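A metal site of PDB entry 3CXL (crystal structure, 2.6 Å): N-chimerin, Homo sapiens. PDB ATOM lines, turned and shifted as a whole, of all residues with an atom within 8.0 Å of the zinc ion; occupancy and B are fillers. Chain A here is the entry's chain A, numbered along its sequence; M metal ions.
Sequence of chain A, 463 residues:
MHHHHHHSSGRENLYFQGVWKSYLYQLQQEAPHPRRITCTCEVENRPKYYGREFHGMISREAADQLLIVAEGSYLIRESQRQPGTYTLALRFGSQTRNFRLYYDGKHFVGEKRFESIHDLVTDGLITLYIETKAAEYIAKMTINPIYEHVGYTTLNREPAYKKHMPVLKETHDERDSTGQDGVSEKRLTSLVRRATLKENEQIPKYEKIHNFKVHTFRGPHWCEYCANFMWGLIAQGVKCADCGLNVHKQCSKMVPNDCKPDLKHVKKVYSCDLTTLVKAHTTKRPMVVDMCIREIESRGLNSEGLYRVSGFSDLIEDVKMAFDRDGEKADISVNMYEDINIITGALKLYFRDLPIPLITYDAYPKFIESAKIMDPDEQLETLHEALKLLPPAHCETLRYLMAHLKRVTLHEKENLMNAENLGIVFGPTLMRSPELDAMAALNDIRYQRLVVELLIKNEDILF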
ATOM      1  N   TYR A 147      -4.062   8.129  -1.258  1.00  0.00           N
ATOM      2  CA  TYR A 147      -3.804   6.777  -0.740  1.00  0.00           C
ATOM      3  C   TYR A 147      -4.493   5.641  -1.467  1.00  0.00           C
ATOM      4  O   TYR A 147      -3.875   4.643  -1.820  1.00  0.00           O
ATOM      5  CB  TYR A 147      -4.219   6.705   0.716  1.00  0.00           C
ATOM      6  CG  TYR A 147      -3.882   5.389   1.372  1.00  0.00           C
ATOM      7  CD1 TYR A 147      -2.556   5.039   1.610  1.00  0.00           C
ATOM      8  CD2 TYR A 147      -4.888   4.514   1.759  1.00  0.00           C
ATOM      9  CE1 TYR A 147      -2.232   3.849   2.207  1.00  0.00           C
ATOM     10  CE2 TYR A 147      -4.570   3.310   2.372  1.00  0.00           C
ATOM     11  CZ  TYR A 147      -3.232   2.982   2.590  1.00  0.00           C
ATOM     12  OH  TYR A 147      -2.907   1.778   3.187  1.00  0.00           O
ATOM     13  N   LYS A 208      -5.736  -5.458   8.822  1.00  0.00           N
ATOM     14  CA  LYS A 208      -4.676  -5.409   9.822  1.00  0.00           C
ATOM     15  C   LYS A 208      -4.391  -3.956  10.164  1.00  0.00           C
ATOM     16  O   LYS A 208      -4.124  -3.134   9.274  1.00  0.00           O
ATOM     17  CB  LYS A 208      -3.401  -6.080   9.318  1.00  0.00           C
ATOM     18  N   ILE A 209      -4.478  -3.645  11.452  1.00  0.00           N
ATOM     19  CA  ILE A 209      -4.140  -2.313  11.921  1.00  0.00           C
ATOM     20  C   ILE A 209      -2.657  -2.127  11.640  1.00  0.00           C
ATOM     21  O   ILE A 209      -1.855  -3.020  11.917  1.00  0.00           O
ATOM     22  CB  ILE A 209      -4.397  -2.144  13.457  1.00  0.00           C
ATOM     23  CG1 ILE A 209      -5.805  -2.622  13.849  1.00  0.00           C
ATOM     24  CG2 ILE A 209      -4.226  -0.700  13.855  1.00  0.00           C
ATOM     25  CD1 ILE A 209      -6.105  -2.520  15.344  1.00  0.00           C
ATOM     26  N   HIS A 210      -2.298  -0.990  11.074  1.00  0.00           N
ATOM     27  CA  HIS A 210      -0.883  -0.717  10.817  1.00  0.00           C
ATOM     28  C   HIS A 210      -0.158  -0.611  12.151  1.00  0.00           C
ATOM     29  O   HIS A 210      -0.767  -0.816  13.206  1.00  0.00           O
ATOM     30  CB  HIS A 210      -0.719   0.564   9.986  1.00  0.00           C
ATOM     31  CG  HIS A 210      -1.080   0.383   8.547  1.00  0.00           C
ATOM     32  ND1 HIS A 210      -0.178  -0.081   7.612  1.00  0.00           N
ATOM     33  CD2 HIS A 210      -2.231   0.597   7.876  1.00  0.00           C
ATOM     34  CE1 HIS A 210      -0.750  -0.145   6.431  1.00  0.00           C
ATOM     35  NE2 HIS A 210      -2.001   0.264   6.563  1.00  0.00           N
ATOM     36  N   ASN A 211       1.142  -0.340  12.101  1.00  0.00           N
ATOM     37  CA  ASN A 211       1.967  -0.204  13.316  1.00  0.00           C
ATOM     38  C   ASN A 211       2.976   0.899  13.077  1.00  0.00           C
ATOM     39  O   ASN A 211       4.128   0.644  12.703  1.00  0.00           O
ATOM     40  CB  ASN A 211       2.657  -1.540  13.660  1.00  0.00           C
ATOM     41  CG  ASN A 211       3.554  -1.455  14.904  1.00  0.00           C
ATOM     42  OD1 ASN A 211       3.458  -0.515  15.698  1.00  0.00           O
ATOM     43  ND2 ASN A 211       4.413  -2.443  15.070  1.00  0.00           N
ATOM     44  N   PHE A 212       2.524   2.130  13.285  1.00  0.00           N
ATOM     45  CA  PHE A 212       3.283   3.318  12.956  1.00  0.00           C
ATOM     46  C   PHE A 212       4.239   3.706  14.067  1.00  0.00           C
ATOM     47  O   PHE A 212       3.834   3.874  15.214  1.00  0.00           O
ATOM     48  CB  PHE A 212       2.329   4.481  12.685  1.00  0.00           C
ATOM     49  CG  PHE A 212       1.532   4.334  11.431  1.00  0.00           C
ATOM     50  CD1 PHE A 212       2.119   4.564  10.177  1.00  0.00           C
ATOM     51  CD2 PHE A 212       0.186   3.981  11.489  1.00  0.00           C
ATOM     52  CE1 PHE A 212       1.383   4.429   9.015  1.00  0.00           C
ATOM     53  CE2 PHE A 212      -0.556   3.838  10.331  1.00  0.00           C
ATOM     54  CZ  PHE A 212       0.049   4.070   9.078  1.00  0.00           C
ATOM     55  N   LYS A 239       6.656   5.845  10.058  1.00  0.00           N
ATOM     56  CA  LYS A 239       6.756   4.763   9.085  1.00  0.00           C
ATOM     57  C   LYS A 239       6.185   3.488   9.703  1.00  0.00           C
ATOM     58  O   LYS A 239       6.327   3.265  10.910  1.00  0.00           O
ATOM     59  CB  LYS A 239       8.215   4.543   8.691  1.00  0.00           C
ATOM     60  CG  LYS A 239       8.449   3.401   7.712  1.00  0.00           C
ATOM     61  CD  LYS A 239       9.916   3.309   7.295  1.00  0.00           C
ATOM     62  CE  LYS A 239      10.073   2.607   5.987  1.00  0.00           C
ATOM     63  NZ  LYS A 239       9.488   3.409   4.880  1.00  0.00           N
ATOM     64  N   CYS A 240       5.528   2.666   8.882  1.00  0.00           N
ATOM     65  CA  CYS A 240       4.966   1.405   9.378  1.00  0.00           C
ATOM     66  C   CYS A 240       6.041   0.343   9.409  1.00  0.00           C
ATOM     67  O   CYS A 240       6.724   0.115   8.416  1.00  0.00           O
ATOM     68  CB  CYS A 240       3.788   0.927   8.519  1.00  0.00           C
ATOM     69  SG  CYS A 240       3.049  -0.605   9.123  1.00  0.00           S
ATOM     70  N   ALA A 241       6.195  -0.298  10.563  1.00  0.00           N
ATOM     71  CA  ALA A 241       7.230  -1.320  10.756  1.00  0.00           C
ATOM     72  C   ALA A 241       6.907  -2.616   9.997  1.00  0.00           C
ATOM     73  O   ALA A 241       7.825  -3.395   9.722  1.00  0.00           O
ATOM     74  CB  ALA A 241       7.431  -1.600  12.234  1.00  0.00           C
ATOM     75  N   ASP A 242       5.634  -2.837   9.668  1.00  0.00           N
ATOM     76  CA  ASP A 242       5.199  -4.064   8.995  1.00  0.00           C
ATOM     77  C   ASP A 242       5.221  -3.956   7.465  1.00  0.00           C
ATOM     78  O   ASP A 242       5.789  -4.832   6.796  1.00  0.00           O
ATOM     79  CB  ASP A 242       3.782  -4.443   9.444  1.00  0.00           C
ATOM     80  CG  ASP A 242       3.689  -4.692  10.931  1.00  0.00           C
ATOM     81  OD1 ASP A 242       4.746  -4.830  11.594  1.00  0.00           O
ATOM     82  OD2 ASP A 242       2.548  -4.762  11.444  1.00  0.00           O
ATOM     83  N   CYS A 243       4.603  -2.906   6.909  1.00  0.00           N
ATOM     84  CA  CYS A 243       4.499  -2.752   5.451  1.00  0.00           C
ATOM     85  C   CYS A 243       5.406  -1.673   4.843  1.00  0.00           C
ATOM     86  O   CYS A 243       5.659  -1.707   3.639  1.00  0.00           O
ATOM     87  CB  CYS A 243       3.059  -2.469   5.040  1.00  0.00           C
ATOM     88  SG  CYS A 243       2.465  -0.844   5.495  1.00  0.00           S
ATOM     89  N   GLY A 244       5.853  -0.714   5.664  1.00  0.00           N
ATOM     90  CA  GLY A 244       6.802   0.333   5.220  1.00  0.00           C
ATOM     91  C   GLY A 244       6.208   1.655   4.716  1.00  0.00           C
ATOM     92  O   GLY A 244       6.953   2.535   4.250  1.00  0.00           O
ATOM     93  N   LEU A 245       4.886   1.794   4.813  1.00  0.00           N
ATOM     94  CA  LEU A 245       4.200   3.017   4.404  1.00  0.00           C
ATOM     95  C   LEU A 245       4.711   4.244   5.137  1.00  0.00           C
ATOM     96  O   LEU A 245       4.823   4.231   6.350  1.00  0.00           O
ATOM     97  CB  LEU A 245       2.708   2.850   4.688  1.00  0.00           C
ATOM     98  CG  LEU A 245       1.770   4.016   4.442  1.00  0.00           C
ATOM     99  CD1 LEU A 245       1.539   4.208   2.928  1.00  0.00           C
ATOM    100  CD2 LEU A 245       0.471   3.783   5.151  1.00  0.00           C
ATOM    101  N   VAL A 255      -5.277   6.610   7.876  1.00  0.00           N
ATOM    102  CA  VAL A 255      -5.006   5.501   6.966  1.00  0.00           C
ATOM    103  C   VAL A 255      -5.835   4.294   7.395  1.00  0.00           C
ATOM    104  O   VAL A 255      -5.798   3.927   8.556  1.00  0.00           O
ATOM    105  CB  VAL A 255      -3.508   5.101   7.001  1.00  0.00           C
ATOM    106  CG1 VAL A 255      -3.246   3.899   6.102  1.00  0.00           C
ATOM    107  CG2 VAL A 255      -2.626   6.285   6.600  1.00  0.00           C
ATOM    108  N   PRO A 256      -6.595   3.690   6.459  1.00  0.00           N
ATOM    109  CA  PRO A 256      -7.356   2.453   6.734  1.00  0.00           C
ATOM    110  C   PRO A 256      -6.526   1.294   7.299  1.00  0.00           C
ATOM    111  O   PRO A 256      -5.293   1.238   7.076  1.00  0.00           O
ATOM    112  CB  PRO A 256      -7.900   2.050   5.358  1.00  0.00           C
ATOM    113  CG  PRO A 256      -7.874   3.283   4.552  1.00  0.00           C
ATOM    114  CD  PRO A 256      -6.797   4.162   5.076  1.00  0.00           C
ATOM    115  N   ASN A 257      -7.197   0.393   8.024  1.00  0.00           N
ATOM    116  CA  ASN A 257      -6.569  -0.841   8.515  1.00  0.00           C
ATOM    117  C   ASN A 257      -6.474  -1.860   7.390  1.00  0.00           C
ATOM    118  O   ASN A 257      -7.202  -2.862   7.353  1.00  0.00           O
ATOM    119  CB  ASN A 257      -7.386  -1.433   9.692  1.00  0.00           C
ATOM    120  CG  ASN A 257      -7.515  -0.473  10.864  1.00  0.00           C
ATOM    121  OD1 ASN A 257      -6.558   0.195  11.238  1.00  0.00           O
ATOM    122  ND2 ASN A 257      -8.701  -0.398  11.419  1.00  0.00           N
ATOM    123  N   ASP A 258      -5.573  -1.572   6.448  1.00  0.00           N
ATOM    124  CA  ASP A 258      -5.357  -2.411   5.276  1.00  0.00           C
ATOM    125  C   ASP A 258      -3.854  -2.775   5.143  1.00  0.00           C
ATOM    126  O   ASP A 258      -3.332  -2.898   4.018  1.00  0.00           O
ATOM    127  CB  ASP A 258      -5.880  -1.704   4.010  1.00  0.00           C
ATOM    128  CG  ASP A 258      -5.127  -0.403   3.690  1.00  0.00           C
ATOM    129  OD1 ASP A 258      -4.173  -0.031   4.432  1.00  0.00           O
ATOM    130  OD2 ASP A 258      -5.505   0.261   2.690  1.00  0.00           O
ATOM    131  N   CYS A 259      -3.187  -2.945   6.283  1.00  0.00           N
ATOM    132  CA  CYS A 259      -1.760  -3.259   6.308  1.00  0.00           C
ATOM    133  C   CYS A 259      -1.455  -4.598   5.601  1.00  0.00           C
ATOM    134  O   CYS A 259      -2.040  -5.649   5.923  1.00  0.00           O
ATOM    135  CB  CYS A 259      -1.252  -3.292   7.742  1.00  0.00           C
ATOM    136  SG  CYS A 259       0.545  -3.437   7.900  1.00  0.00           S
ATOM    137  N   LYS A 260      -0.556  -4.516   4.613  1.00  0.00           N
ATOM    138  CA  LYS A 260      -0.089  -5.678   3.858  1.00  0.00           C
ATOM    139  C   LYS A 260       1.437  -5.805   4.035  1.00  0.00           C
ATOM    140  O   LYS A 260       2.197  -5.209   3.275  1.00  0.00           O
ATOM    141  CB  LYS A 260      -0.464  -5.534   2.386  1.00  0.00           C
ATOM    142  CG  LYS A 260      -1.985  -5.464   2.127  1.00  0.00           C
ATOM    143  CD  LYS A 260      -2.700  -6.739   2.586  1.00  0.00           C
ATOM    144  CE  LYS A 260      -4.183  -6.708   2.273  1.00  0.00           C
ATOM    145  NZ  LYS A 260      -4.882  -7.839   2.947  1.00  0.00           N
ATOM    146  N   PRO A 261       1.881  -6.570   5.061  1.00  0.00           N
ATOM    147  CA  PRO A 261       3.306  -6.669   5.447  1.00  0.00           C
ATOM    148  C   PRO A 261       4.305  -7.083   4.348  1.00  0.00           C
ATOM    149  O   PRO A 261       5.489  -6.758   4.457  1.00  0.00           O
ATOM    150  CB  PRO A 261       3.295  -7.708   6.570  1.00  0.00           C
ATOM    151  CG  PRO A 261       1.929  -7.635   7.127  1.00  0.00           C
ATOM    152  CD  PRO A 261       1.035  -7.365   5.965  1.00  0.00           C
ATOM    153  N   LEU A 263       4.534  -5.784   1.560  1.00  0.00           N
ATOM    154  CA  LEU A 263       4.938  -4.524   0.936  1.00  0.00           C
ATOM    155  C   LEU A 263       6.312  -4.009   1.422  1.00  0.00           C
ATOM    156  O   LEU A 263       6.970  -3.237   0.711  1.00  0.00           O
ATOM    157  CB  LEU A 263       3.852  -3.447   1.166  1.00  0.00           C
ATOM    158  N   LYS A 264       6.740  -4.420   2.611  1.00  0.00           N
ATOM    159  CA  LYS A 264       8.095  -4.078   3.095  1.00  0.00           C
ATOM    160  C   LYS A 264       9.138  -4.558   2.089  1.00  0.00           C
ATOM    161  O   LYS A 264       9.979  -3.790   1.643  1.00  0.00           O
ATOM    162  CB  LYS A 264       8.357  -4.701   4.474  1.00  0.00           C
HETATM  163 ZN    ZN M   1       1.478  -1.312   7.555  1.00  0.00          ZN
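Within 4 Å of the zinc ion: His 210, Cys 240, Cys 243 and Cys 259.
The nearest printed residue that does not touch the zinc ion is Asp 242 (4.3 Å).
The backbone carbonyl oxygen (O) of Cys 243 sits at hydrogen-bond distance from the backbone NH (N) of Lys 264 (3.1 Å).
The side-chain sulfur (SG) of Cys 240 sits close to the backbone NH (N) of Asn 211, 3.5 Å away.
A ring nitrogen (NE2) of His 210 lies close to the backbone carbonyl oxygen (O) of Pro 256 (3.5 Å).
SG of Cys 240 sits close to N of Asp 242 (3.5 Å).
The backbone NH of Cys 259 is in hydrogen-bond range of the backbone carbonyl oxygen of Lys 208.
A ring nitrogen (NE2) of His 210 lies within hydrogen-bond range of the side-chain carboxylate (OD1) of Asp 258.
N of Cys 240 lies within hydrogen-bond range of O of Leu 245 (3.1 Å).
SG of Cys 243 lies close to N of Leu 245, 3.6 Å away.
A ring nitrogen (ND1) of His 210 is bound to the zinc ion (2.1 Å).
The side-chain sulfur (SG) of Cys 240 is bound to the zinc ion (2.3 Å).
The side-chain sulfur (SG) of Cys 243 binds the zinc ion.
The side-chain sulfur (SG) of Cys 259 binds the zinc ion, at 2.3 Å.
The zinc ion has four donor atoms within binding distance.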
